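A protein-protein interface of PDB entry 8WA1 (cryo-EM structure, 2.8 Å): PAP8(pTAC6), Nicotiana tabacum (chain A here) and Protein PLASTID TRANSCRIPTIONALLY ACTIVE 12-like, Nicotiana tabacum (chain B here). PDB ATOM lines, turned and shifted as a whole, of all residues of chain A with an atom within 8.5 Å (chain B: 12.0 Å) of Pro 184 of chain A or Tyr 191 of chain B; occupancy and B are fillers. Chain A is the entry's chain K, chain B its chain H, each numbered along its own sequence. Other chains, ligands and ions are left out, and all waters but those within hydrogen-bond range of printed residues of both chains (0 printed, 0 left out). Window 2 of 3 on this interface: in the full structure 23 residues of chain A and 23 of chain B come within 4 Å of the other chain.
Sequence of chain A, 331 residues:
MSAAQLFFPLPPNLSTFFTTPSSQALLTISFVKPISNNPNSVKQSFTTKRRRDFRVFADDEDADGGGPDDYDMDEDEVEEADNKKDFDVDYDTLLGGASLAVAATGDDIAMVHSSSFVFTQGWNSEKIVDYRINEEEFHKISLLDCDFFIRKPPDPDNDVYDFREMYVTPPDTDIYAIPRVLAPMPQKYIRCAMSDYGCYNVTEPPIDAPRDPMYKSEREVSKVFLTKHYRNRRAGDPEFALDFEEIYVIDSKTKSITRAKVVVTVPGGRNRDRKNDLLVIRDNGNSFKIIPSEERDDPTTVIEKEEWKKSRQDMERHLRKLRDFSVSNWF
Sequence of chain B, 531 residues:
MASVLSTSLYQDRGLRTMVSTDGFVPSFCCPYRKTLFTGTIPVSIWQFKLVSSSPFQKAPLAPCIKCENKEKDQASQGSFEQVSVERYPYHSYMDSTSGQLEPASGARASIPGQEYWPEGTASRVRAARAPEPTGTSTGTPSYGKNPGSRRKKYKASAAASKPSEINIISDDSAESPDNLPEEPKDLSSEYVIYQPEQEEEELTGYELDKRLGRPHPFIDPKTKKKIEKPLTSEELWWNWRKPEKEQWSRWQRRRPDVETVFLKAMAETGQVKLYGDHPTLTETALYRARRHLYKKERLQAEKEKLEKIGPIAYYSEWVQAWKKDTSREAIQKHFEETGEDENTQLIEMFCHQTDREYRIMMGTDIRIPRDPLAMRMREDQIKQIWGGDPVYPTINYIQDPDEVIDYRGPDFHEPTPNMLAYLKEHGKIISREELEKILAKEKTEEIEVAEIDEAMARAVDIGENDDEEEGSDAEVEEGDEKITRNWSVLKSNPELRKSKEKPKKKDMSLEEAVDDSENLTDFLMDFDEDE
Ala 183 of chain A touches just one residue of chain B: Tyr 191 (3.3 Å).
No residue of chain B comes within 4 Å of Met 185 of chain A.
No residue of chain B comes within 4 Å of Thr 258 of chain A.
Ala 260 of chain A touches just one residue of chain B: Tyr 191 (3.4 Å).
Lys 261 of chain A touches just these residues of chain B: Glu 190 (3.6 Å) and Tyr 191 (3.5 Å).
Val 262 of chain A touches two residues of chain B.
Printed residues of chain A within 4 Å of Tyr 194 of chain B: Glu 245 and Val 264.
Of the printed residues of chain B, Val 264 of chain A touches Ile 193, Tyr 194 and Gln 195.
Of the printed residues of chain A, Glu 190 of chain B touches Lys 261.
The nearest residue of chain A that does not touch Tyr 191 of chain B is Leu 182 of chain A (4.5 Å).
The nearest printed residue of chain B that does not touch Val 264 of chain A is Val 192 of chain B (4.3 Å).
Among the printed residues, pairs that only touch across the chains: Ala 183 of chain A with Tyr 191 of chain B, Pro 184 of chain A with Tyr 191 of chain B, Glu 245 of chain A with Val 192 of chain B, Glu 245 of chain A with Tyr 194 of chain B, Arg 259 of chain A with Tyr 191 of chain B, Arg 259 of chain A with Val 192 of chain B, Ala 260 of chain A with Tyr 191 of chain B, Lys 261 of chain A with Tyr 191 of chain B, Val 263 of chain A with Ile 193 of chain B, Val 263 of chain A with Gln 195 of chain B and Val 264 of chain A with Tyr 194 of chain B.
The guanidinium group of Arg 259 of chain A sits at hydrogen-bond distance from the backbone carbonyl oxygen of Glu 245 of chain A, at 3.0 Å.
The backbone carbonyl oxygen (O) of Ile 247 of chain A sits at hydrogen-bond distance from the backbone NH (N) of Ala 260 of chain A (2.7 Å).
The backbone carbonyl oxygen (O) of Phe 288 of chain A lies within hydrogen-bond range of the backbone NH (N) of Val 263 of chain A (3.0 Å).
The side-chain amino group (NZ) of Lys 261 of chain A lies within salt-bridge range of the side-chain carboxylate (OE2) of Glu 190 of chain B (3.6 Å).
The backbone NH (N) of Val 262 of chain A sits at hydrogen-bond distance from the backbone carbonyl oxygen (O) of Tyr 191 of chain B (3.3 Å).
O of Val 262 of chain A is in hydrogen-bond range of N of Ile 193 of chain B (3.1 Å).
The backbone carbonyl oxygen of Ile 193 of chain B sits at hydrogen-bond distance from the backbone NH of Val 264 of chain A (2.9 Å).
The backbone NH (N) of Gln 195 of chain B is in hydrogen-bond range of the backbone carbonyl oxygen (O) of Val 264 of chain A.
Of the 9 printed residues of chain B, 6 touch a printed residue of chain A.
Hydrophobic or aromatic side chains of chain B that line the printed part of chain A: Tyr 191, Val 192, Ile 193 and Tyr 194.
Of the 23 printed residues of chain A, 9 touch a printed residue of chain B.
Hydrophobic or aromatic side chains of chain A that line the printed part of chain B: Ala 183, Pro 184, Val 263 and Val 264.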
ATOM      1  N   PHE A 163      -2.258   3.099   5.945  1.00  0.00           N
ATOM      2  CA  PHE A 163      -1.615   1.794   6.009  1.00  0.00           C
ATOM      3  C   PHE A 163      -0.096   1.867   5.937  1.00  0.00           C
ATOM      4  O   PHE A 163       0.557   0.818   5.927  1.00  0.00           O
ATOM      5  CB  PHE A 163      -2.139   0.895   4.885  1.00  0.00           C
ATOM      6  CG  PHE A 163      -3.564   0.457   5.073  1.00  0.00           C
ATOM      7  CD1 PHE A 163      -4.614   1.292   4.731  1.00  0.00           C
ATOM      8  CD2 PHE A 163      -3.853  -0.796   5.590  1.00  0.00           C
ATOM      9  CE1 PHE A 163      -5.924   0.890   4.902  1.00  0.00           C
ATOM     10  CE2 PHE A 163      -5.161  -1.204   5.764  1.00  0.00           C
ATOM     11  CZ  PHE A 163      -6.198  -0.361   5.419  1.00  0.00           C
ATOM     12  N   MET A 166       1.805   0.647  10.646  1.00  0.00           N
ATOM     13  CA  MET A 166       0.917  -0.305  11.299  1.00  0.00           C
ATOM     14  C   MET A 166       1.729  -1.162  12.256  1.00  0.00           C
ATOM     15  O   MET A 166       2.902  -1.458  12.007  1.00  0.00           O
ATOM     16  CB  MET A 166       0.183  -1.184  10.279  1.00  0.00           C
ATOM     17  CG  MET A 166       1.099  -1.900   9.302  1.00  0.00           C
ATOM     18  SD  MET A 166       0.203  -2.998   8.188  1.00  0.00           S
ATOM     19  CE  MET A 166      -0.920  -1.841   7.407  1.00  0.00           C
ATOM     20  N   VAL A 181       3.363  -8.035   6.370  1.00  0.00           N
ATOM     21  CA  VAL A 181       2.723  -7.491   5.178  1.00  0.00           C
ATOM     22  C   VAL A 181       2.825  -8.515   4.056  1.00  0.00           C
ATOM     23  O   VAL A 181       3.870  -8.641   3.406  1.00  0.00           O
ATOM     24  CB  VAL A 181       3.353  -6.148   4.768  1.00  0.00           C
ATOM     25  CG1 VAL A 181       2.679  -5.604   3.518  1.00  0.00           C
ATOM     26  CG2 VAL A 181       3.252  -5.147   5.908  1.00  0.00           C
ATOM     27  N   LEU A 182       1.745  -9.258   3.826  1.00  0.00           N
ATOM     28  CA  LEU A 182       1.724 -10.322   2.832  1.00  0.00           C
ATOM     29  C   LEU A 182       1.071  -9.906   1.521  1.00  0.00           C
ATOM     30  O   LEU A 182       0.870 -10.759   0.650  1.00  0.00           O
ATOM     31  CB  LEU A 182       1.005 -11.551   3.396  1.00  0.00           C
ATOM     32  CG  LEU A 182       1.583 -12.131   4.687  1.00  0.00           C
ATOM     33  CD1 LEU A 182       0.833 -13.389   5.093  1.00  0.00           C
ATOM     34  CD2 LEU A 182       3.071 -12.414   4.533  1.00  0.00           C
ATOM     35  N   ALA A 183       0.733  -8.633   1.358  1.00  0.00           N
ATOM     36  CA  ALA A 183       0.098  -8.156   0.138  1.00  0.00           C
ATOM     37  C   ALA A 183       0.446  -6.686  -0.033  1.00  0.00           C
ATOM     38  O   ALA A 183       0.730  -5.989   0.951  1.00  0.00           O
ATOM     39  CB  ALA A 183      -1.427  -8.360   0.182  1.00  0.00           C
ATOM     40  N   PRO A 184       0.449  -6.186  -1.269  1.00  0.00           N
ATOM     41  CA  PRO A 184       0.688  -4.753  -1.476  1.00  0.00           C
ATOM     42  C   PRO A 184      -0.374  -3.914  -0.782  1.00  0.00           C
ATOM     43  O   PRO A 184      -1.567  -4.024  -1.070  1.00  0.00           O
ATOM     44  CB  PRO A 184       0.622  -4.601  -3.000  1.00  0.00           C
ATOM     45  CG  PRO A 184       0.968  -5.952  -3.525  1.00  0.00           C
ATOM     46  CD  PRO A 184       0.391  -6.926  -2.541  1.00  0.00           C
ATOM     47  N   MET A 185       0.078  -3.071   0.143  1.00  0.00           N
ATOM     48  CA  MET A 185      -0.817  -2.255   0.942  1.00  0.00           C
ATOM     49  C   MET A 185      -0.999  -0.882   0.309  1.00  0.00           C
ATOM     50  O   MET A 185      -0.067  -0.361  -0.316  1.00  0.00           O
ATOM     51  CB  MET A 185      -0.282  -2.090   2.370  1.00  0.00           C
ATOM     52  CG  MET A 185      -0.287  -3.367   3.199  1.00  0.00           C
ATOM     53  SD  MET A 185      -1.943  -3.946   3.626  1.00  0.00           S
ATOM     54  CE  MET A 185      -2.154  -5.292   2.463  1.00  0.00           C
ATOM     55  N   PRO A 186      -2.180  -0.281   0.441  1.00  0.00           N
ATOM     56  CA  PRO A 186      -2.403   1.044  -0.148  1.00  0.00           C
ATOM     57  C   PRO A 186      -1.507   2.093   0.493  1.00  0.00           C
ATOM     58  O   PRO A 186      -1.414   2.196   1.718  1.00  0.00           O
ATOM     59  CB  PRO A 186      -3.884   1.314   0.137  1.00  0.00           C
ATOM     60  CG  PRO A 186      -4.201   0.457   1.317  1.00  0.00           C
ATOM     61  CD  PRO A 186      -3.366  -0.776   1.161  1.00  0.00           C
ATOM     62  N   GLN A 187      -0.843   2.874  -0.355  1.00  0.00           N
ATOM     63  CA  GLN A 187       0.087   3.902   0.088  1.00  0.00           C
ATOM     64  C   GLN A 187      -0.548   5.286   0.125  1.00  0.00           C
ATOM     65  O   GLN A 187       0.163   6.282   0.302  1.00  0.00           O
ATOM     66  CB  GLN A 187       1.327   3.908  -0.809  1.00  0.00           C
ATOM     67  CG  GLN A 187       2.058   2.573  -0.846  1.00  0.00           C
ATOM     68  CD  GLN A 187       3.184   2.544  -1.863  1.00  0.00           C
ATOM     69  OE1 GLN A 187       3.435   3.527  -2.560  1.00  0.00           O
ATOM     70  NE2 GLN A 187       3.870   1.410  -1.951  1.00  0.00           N
ATOM     71  N   PHE A 244     -16.378  -3.556  -3.077  1.00  0.00           N
ATOM     72  CA  PHE A 244     -16.140  -4.943  -2.702  1.00  0.00           C
ATOM     73  C   PHE A 244     -14.978  -5.568  -3.464  1.00  0.00           C
ATOM     74  O   PHE A 244     -14.761  -6.779  -3.360  1.00  0.00           O
ATOM     75  CB  PHE A 244     -17.409  -5.769  -2.912  1.00  0.00           C
ATOM     76  CG  PHE A 244     -18.520  -5.430  -1.961  1.00  0.00           C
ATOM     77  CD1 PHE A 244     -18.242  -4.979  -0.682  1.00  0.00           C
ATOM     78  CD2 PHE A 244     -19.843  -5.560  -2.346  1.00  0.00           C
ATOM     79  CE1 PHE A 244     -19.262  -4.668   0.196  1.00  0.00           C
ATOM     80  CE2 PHE A 244     -20.867  -5.249  -1.476  1.00  0.00           C
ATOM     81  CZ  PHE A 244     -20.577  -4.803  -0.203  1.00  0.00           C
ATOM     82  N   GLU A 245     -14.229  -4.771  -4.223  1.00  0.00           N
ATOM     83  CA  GLU A 245     -13.066  -5.258  -4.947  1.00  0.00           C
ATOM     84  C   GLU A 245     -11.764  -5.034  -4.193  1.00  0.00           C
ATOM     85  O   GLU A 245     -10.729  -5.570  -4.603  1.00  0.00           O
ATOM     86  CB  GLU A 245     -12.984  -4.584  -6.322  1.00  0.00           C
ATOM     87  CG  GLU A 245     -14.242  -4.747  -7.158  1.00  0.00           C
ATOM     88  CD  GLU A 245     -14.177  -3.989  -8.469  1.00  0.00           C
ATOM     89  OE1 GLU A 245     -15.201  -3.944  -9.184  1.00  0.00           O
ATOM     90  OE2 GLU A 245     -13.103  -3.436  -8.784  1.00  0.00           O
ATOM     91  N   GLU A 246     -11.790  -4.262  -3.106  1.00  0.00           N
ATOM     92  CA  GLU A 246     -10.603  -3.957  -2.306  1.00  0.00           C
ATOM     93  C   GLU A 246     -10.937  -4.271  -0.849  1.00  0.00           C
ATOM     94  O   GLU A 246     -11.409  -3.410  -0.103  1.00  0.00           O
ATOM     95  CB  GLU A 246     -10.176  -2.507  -2.503  1.00  0.00           C
ATOM     96  CG  GLU A 246      -8.905  -2.124  -1.771  1.00  0.00           C
ATOM     97  CD  GLU A 246      -8.416  -0.740  -2.145  1.00  0.00           C
ATOM     98  OE1 GLU A 246      -8.823  -0.238  -3.212  1.00  0.00           O
ATOM     99  OE2 GLU A 246      -7.630  -0.153  -1.372  1.00  0.00           O
ATOM    100  N   ILE A 247     -10.692  -5.516  -0.451  1.00  0.00           N
ATOM    101  CA  ILE A 247     -10.967  -5.992   0.899  1.00  0.00           C
ATOM    102  C   ILE A 247      -9.645  -6.369   1.551  1.00  0.00           C
ATOM    103  O   ILE A 247      -8.852  -7.120   0.970  1.00  0.00           O
ATOM    104  CB  ILE A 247     -11.932  -7.190   0.889  1.00  0.00           C
ATOM    105  CG1 ILE A 247     -13.176  -6.871   0.055  1.00  0.00           C
ATOM    106  CG2 ILE A 247     -12.321  -7.572   2.308  1.00  0.00           C
ATOM    107  CD1 ILE A 247     -13.973  -5.694   0.569  1.00  0.00           C
ATOM    108  N   TYR A 248      -9.410  -5.850   2.752  1.00  0.00           N
ATOM    109  CA  TYR A 248      -8.221  -6.173   3.530  1.00  0.00           C
ATOM    110  C   TYR A 248      -8.643  -6.922   4.784  1.00  0.00           C
ATOM    111  O   TYR A 248      -9.472  -6.429   5.557  1.00  0.00           O
ATOM    112  CB  TYR A 248      -7.438  -4.911   3.900  1.00  0.00           C
ATOM    113  CG  TYR A 248      -7.027  -4.076   2.708  1.00  0.00           C
ATOM    114  CD1 TYR A 248      -5.963  -4.459   1.902  1.00  0.00           C
ATOM    115  CD2 TYR A 248      -7.698  -2.902   2.394  1.00  0.00           C
ATOM    116  CE1 TYR A 248      -5.583  -3.698   0.814  1.00  0.00           C
ATOM    117  CE2 TYR A 248      -7.324  -2.134   1.309  1.00  0.00           C
ATOM    118  CZ  TYR A 248      -6.266  -2.539   0.522  1.00  0.00           C
ATOM    119  OH  TYR A 248      -5.889  -1.779  -0.562  1.00  0.00           O
ATOM    120  N   ILE A 257      -1.688  -9.088   7.850  1.00  0.00           N
ATOM    121  CA  ILE A 257      -2.722  -8.379   7.107  1.00  0.00           C
ATOM    122  C   ILE A 257      -2.459  -8.580   5.620  1.00  0.00           C
ATOM    123  O   ILE A 257      -1.332  -8.384   5.150  1.00  0.00           O
ATOM    124  CB  ILE A 257      -2.758  -6.883   7.471  1.00  0.00           C
ATOM    125  CG1 ILE A 257      -3.701  -6.127   6.532  1.00  0.00           C
ATOM    126  CG2 ILE A 257      -1.358  -6.283   7.451  1.00  0.00           C
ATOM    127  CD1 ILE A 257      -3.819  -4.653   6.844  1.00  0.00           C
ATOM    128  N   THR A 258      -3.491  -8.991   4.887  1.00  0.00           N
ATOM    129  CA  THR A 258      -3.369  -9.253   3.462  1.00  0.00           C
ATOM    130  C   THR A 258      -4.632  -8.788   2.751  1.00  0.00           C
ATOM    131  O   THR A 258      -5.628  -8.418   3.378  1.00  0.00           O
ATOM    132  CB  THR A 258      -3.110 -10.740   3.181  1.00  0.00           C
ATOM    133  OG1 THR A 258      -3.334 -11.012   1.792  1.00  0.00           O
ATOM    134  CG2 THR A 258      -4.028 -11.611   4.024  1.00  0.00           C
ATOM    135  N   ARG A 259      -4.577  -8.809   1.423  1.00  0.00           N
ATOM    136  CA  ARG A 259      -5.678  -8.375   0.577  1.00  0.00           C
ATOM    137  C   ARG A 259      -6.466  -9.588   0.102  1.00  0.00           C
ATOM    138  O   ARG A 259      -5.883 -10.597  -0.309  1.00  0.00           O
ATOM    139  CB  ARG A 259      -5.160  -7.578  -0.624  1.00  0.00           C
ATOM    140  CG  ARG A 259      -6.208  -6.732  -1.326  1.00  0.00           C
ATOM    141  CD  ARG A 259      -5.579  -5.926  -2.452  1.00  0.00           C
ATOM    142  NE  ARG A 259      -6.484  -4.919  -2.998  1.00  0.00           N
ATOM    143  CZ  ARG A 259      -7.292  -5.122  -4.032  1.00  0.00           C
ATOM    144  NH1 ARG A 259      -7.315  -6.300  -4.638  1.00  0.00           N
ATOM    145  NH2 ARG A 259      -8.079  -4.146  -4.462  1.00  0.00           N
ATOM    146  N   ALA A 260      -7.790  -9.486   0.163  1.00  0.00           N
ATOM    147  CA  ALA A 260      -8.644 -10.601  -0.212  1.00  0.00           C
ATOM    148  C   ALA A 260      -8.735 -10.730  -1.729  1.00  0.00           C
ATOM    149  O   ALA A 260      -8.534  -9.771  -2.480  1.00  0.00           O
ATOM    150  CB  ALA A 260     -10.041 -10.430   0.383  1.00  0.00           C
ATOM    151  N   LYS A 261      -9.046 -11.943  -2.178  1.00  0.00           N
ATOM    152  CA  LYS A 261      -9.251 -12.241  -3.591  1.00  0.00           C
ATOM    153  C   LYS A 261     -10.739 -12.452  -3.832  1.00  0.00           C
ATOM    154  O   LYS A 261     -11.315 -13.437  -3.355  1.00  0.00           O
ATOM    155  CB  LYS A 261      -8.460 -13.478  -4.016  1.00  0.00           C
ATOM    156  CG  LYS A 261      -6.953 -13.322  -3.929  1.00  0.00           C
ATOM    157  CD  LYS A 261      -6.246 -14.485  -4.604  1.00  0.00           C
ATOM    158  CE  LYS A 261      -4.736 -14.315  -4.573  1.00  0.00           C
ATOM    159  NZ  LYS A 261      -4.045 -15.355  -5.383  1.00  0.00           N
ATOM    160  N   VAL A 262     -11.355 -11.535  -4.569  1.00  0.00           N
ATOM    161  CA  VAL A 262     -12.779 -11.599  -4.873  1.00  0.00           C
ATOM    162  C   VAL A 262     -12.956 -12.119  -6.291  1.00  0.00           C
ATOM    163  O   VAL A 262     -12.055 -12.021  -7.132  1.00  0.00           O
ATOM    164  CB  VAL A 262     -13.464 -10.226  -4.699  1.00  0.00           C
ATOM    165  CG1 VAL A 262     -13.242  -9.699  -3.291  1.00  0.00           C
ATOM    166  CG2 VAL A 262     -12.946  -9.236  -5.732  1.00  0.00           C
ATOM    167  N   VAL A 263     -14.132 -12.689  -6.552  1.00  0.00           N
ATOM    168  CA  VAL A 263     -14.453 -13.232  -7.868  1.00  0.00           C
ATOM    169  C   VAL A 263     -15.712 -12.553  -8.385  1.00  0.00           C
ATOM    170  O   VAL A 263     -16.831 -12.977  -8.076  1.00  0.00           O
ATOM    171  CB  VAL A 263     -14.629 -14.759  -7.818  1.00  0.00           C
ATOM    172  CG1 VAL A 263     -14.831 -15.316  -9.219  1.00  0.00           C
ATOM    173  CG2 VAL A 263     -13.432 -15.412  -7.145  1.00  0.00           C
ATOM    174  N   VAL A 264     -15.537 -11.491  -9.175  1.00  0.00           N
ATOM    175  CA  VAL A 264     -16.682 -10.758  -9.698  1.00  0.00           C
ATOM    176  C   VAL A 264     -17.425 -11.622 -10.705  1.00  0.00           C
ATOM    177  O   VAL A 264     -16.845 -12.103 -11.687  1.00  0.00           O
ATOM    178  CB  VAL A 264     -16.228  -9.434 -10.329  1.00  0.00           C
ATOM    179  CG1 VAL A 264     -17.429  -8.660 -10.842  1.00  0.00           C
ATOM    180  CG2 VAL A 264     -15.443  -8.608  -9.323  1.00  0.00           C
ATOM    181  N   PHE A 288     -14.472 -15.127  -1.363  1.00  0.00           N
ATOM    182  CA  PHE A 288     -15.172 -13.868  -1.580  1.00  0.00           C
ATOM    183  C   PHE A 288     -15.732 -13.848  -2.995  1.00  0.00           C
ATOM    184  O   PHE A 288     -14.988 -14.037  -3.963  1.00  0.00           O
ATOM    185  CB  PHE A 288     -14.240 -12.674  -1.362  1.00  0.00           C
ATOM    186  CG  PHE A 288     -13.678 -12.589   0.028  1.00  0.00           C
ATOM    187  CD1 PHE A 288     -12.497 -13.235   0.351  1.00  0.00           C
ATOM    188  CD2 PHE A 288     -14.327 -11.858   1.009  1.00  0.00           C
ATOM    189  CE1 PHE A 288     -11.976 -13.158   1.628  1.00  0.00           C
ATOM    190  CE2 PHE A 288     -13.810 -11.776   2.287  1.00  0.00           C
ATOM    191  CZ  PHE A 288     -12.633 -12.427   2.598  1.00  0.00           C
ATOM    192  N   LEU B 187      -4.740  -5.075 -16.987  1.00  0.00           N
ATOM    193  CA  LEU B 187      -5.341  -4.034 -16.162  1.00  0.00           C
ATOM    194  C   LEU B 187      -5.879  -4.612 -14.858  1.00  0.00           C
ATOM    195  O   LEU B 187      -5.743  -4.005 -13.796  1.00  0.00           O
ATOM    196  CB  LEU B 187      -6.460  -3.324 -16.927  1.00  0.00           C
ATOM    197  CG  LEU B 187      -7.182  -2.194 -16.189  1.00  0.00           C
ATOM    198  CD1 LEU B 187      -6.208  -1.087 -15.814  1.00  0.00           C
ATOM    199  CD2 LEU B 187      -8.325  -1.646 -17.031  1.00  0.00           C
ATOM    200  N   SER B 188      -6.492  -5.789 -14.949  1.00  0.00           N
ATOM    201  CA  SER B 188      -7.040  -6.442 -13.767  1.00  0.00           C
ATOM    202  C   SER B 188      -5.920  -6.894 -12.838  1.00  0.00           C
ATOM    203  O   SER B 188      -4.867  -7.356 -13.284  1.00  0.00           O
ATOM    204  CB  SER B 188      -7.901  -7.637 -14.172  1.00  0.00           C
ATOM    205  OG  SER B 188      -7.119  -8.644 -14.790  1.00  0.00           O
ATOM    206  N   SER B 189      -6.153  -6.755 -11.535  1.00  0.00           N
ATOM    207  CA  SER B 189      -5.159  -7.124 -10.543  1.00  0.00           C
ATOM    208  C   SER B 189      -5.193  -8.630 -10.280  1.00  0.00           C
ATOM    209  O   SER B 189      -6.097  -9.348 -10.717  1.00  0.00           O
ATOM    210  CB  SER B 189      -5.387  -6.350  -9.246  1.00  0.00           C
ATOM    211  OG  SER B 189      -5.264  -4.953  -9.458  1.00  0.00           O
ATOM    212  N   GLU B 190      -4.179  -9.105  -9.553  1.00  0.00           N
ATOM    213  CA  GLU B 190      -4.110 -10.523  -9.209  1.00  0.00           C
ATOM    214  C   GLU B 190      -5.278 -10.935  -8.322  1.00  0.00           C
ATOM    215  O   GLU B 190      -5.762 -12.070  -8.405  1.00  0.00           O
ATOM    216  CB  GLU B 190      -2.780 -10.827  -8.516  1.00  0.00           C
ATOM    217  CG  GLU B 190      -2.643 -12.258  -8.019  1.00  0.00           C
ATOM    218  CD  GLU B 190      -1.396 -12.473  -7.184  1.00  0.00           C
ATOM    219  OE1 GLU B 190      -0.650 -11.497  -6.963  1.00  0.00           O
ATOM    220  OE2 GLU B 190      -1.163 -13.621  -6.748  1.00  0.00           O
ATOM    221  N   TYR B 191      -5.747 -10.025  -7.469  1.00  0.00           N
ATOM    222  CA  TYR B 191      -6.794 -10.372  -6.515  1.00  0.00           C
ATOM    223  C   TYR B 191      -8.177 -10.269  -7.147  1.00  0.00           C
ATOM    224  O   TYR B 191      -9.053 -11.103  -6.885  1.00  0.00           O
ATOM    225  CB  TYR B 191      -6.690  -9.474  -5.282  1.00  0.00           C
ATOM    226  CG  TYR B 191      -5.310  -9.464  -4.658  1.00  0.00           C
ATOM    227  CD1 TYR B 191      -4.953 -10.399  -3.695  1.00  0.00           C
ATOM    228  CD2 TYR B 191      -4.363  -8.522  -5.037  1.00  0.00           C
ATOM    229  CE1 TYR B 191      -3.693 -10.394  -3.127  1.00  0.00           C
ATOM    230  CE2 TYR B 191      -3.101  -8.510  -4.475  1.00  0.00           C
ATOM    231  CZ  TYR B 191      -2.772  -9.448  -3.520  1.00  0.00           C
ATOM    232  OH  TYR B 191      -1.516  -9.440  -2.958  1.00  0.00           O
ATOM    233  N   VAL B 192      -8.396  -9.256  -7.983  1.00  0.00           N
ATOM    234  CA  VAL B 192      -9.704  -9.030  -8.589  1.00  0.00           C
ATOM    235  C   VAL B 192      -9.878  -9.933  -9.801  1.00  0.00           C
ATOM    236  O   VAL B 192      -9.475  -9.584 -10.917  1.00  0.00           O
ATOM    237  CB  VAL B 192      -9.890  -7.550  -8.973  1.00  0.00           C
ATOM    238  CG1 VAL B 192     -11.296  -7.316  -9.497  1.00  0.00           C
ATOM    239  CG2 VAL B 192      -9.607  -6.653  -7.778  1.00  0.00           C
ATOM    240  N   ILE B 193     -10.473 -11.107  -9.589  1.00  0.00           N
ATOM    241  CA  ILE B 193     -10.735 -12.030 -10.685  1.00  0.00           C
ATOM    242  C   ILE B 193     -12.096 -11.721 -11.303  1.00  0.00           C
ATOM    243  O   ILE B 193     -13.007 -11.207 -10.648  1.00  0.00           O
ATOM    244  CB  ILE B 193     -10.655 -13.489 -10.196  1.00  0.00           C
ATOM    245  CG1 ILE B 193      -9.380 -13.702  -9.376  1.00  0.00           C
ATOM    246  CG2 ILE B 193     -10.670 -14.465 -11.365  1.00  0.00           C
ATOM    247  CD1 ILE B 193      -8.108 -13.474 -10.162  1.00  0.00           C
ATOM    248  N   TYR B 194     -12.234 -12.046 -12.588  1.00  0.00           N
ATOM    249  CA  TYR B 194     -13.473 -11.825 -13.322  1.00  0.00           C
ATOM    250  C   TYR B 194     -13.904 -13.119 -13.991  1.00  0.00           C
ATOM    251  O   TYR B 194     -13.199 -13.632 -14.865  1.00  0.00           O
ATOM    252  CB  TYR B 194     -13.310 -10.723 -14.376  1.00  0.00           C
ATOM    253  CG  TYR B 194     -13.500  -9.322 -13.843  1.00  0.00           C
ATOM    254  CD1 TYR B 194     -12.430  -8.599 -13.335  1.00  0.00           C
ATOM    255  CD2 TYR B 194     -14.752  -8.719 -13.855  1.00  0.00           C
ATOM    256  CE1 TYR B 194     -12.601  -7.318 -12.850  1.00  0.00           C
ATOM    257  CE2 TYR B 194     -14.932  -7.439 -13.372  1.00  0.00           C
ATOM    258  CZ  TYR B 194     -13.854  -6.742 -12.870  1.00  0.00           C
ATOM    259  OH  TYR B 194     -14.032  -5.467 -12.388  1.00  0.00           O
ATOM    260  N   GLN B 195     -15.059 -13.640 -13.583  1.00  0.00           N
ATOM    261  CA  GLN B 195     -15.647 -14.845 -14.170  1.00  0.00           C
ATOM    262  C   GLN B 195     -17.118 -14.582 -14.466  1.00  0.00           C
ATOM    263  O   GLN B 195     -18.007 -15.108 -13.786  1.00  0.00           O
ATOM    264  CB  GLN B 195     -15.479 -16.049 -13.243  1.00  0.00           C
ATOM    265  CG  GLN B 195     -14.033 -16.419 -12.952  1.00  0.00           C
ATOM    266  CD  GLN B 195     -13.913 -17.626 -12.043  1.00  0.00           C
ATOM    267  OE1 GLN B 195     -12.809 -18.053 -11.702  1.00  0.00           O
ATOM    268  NE2 GLN B 195     -15.051 -18.183 -11.645  1.00  0.00           N
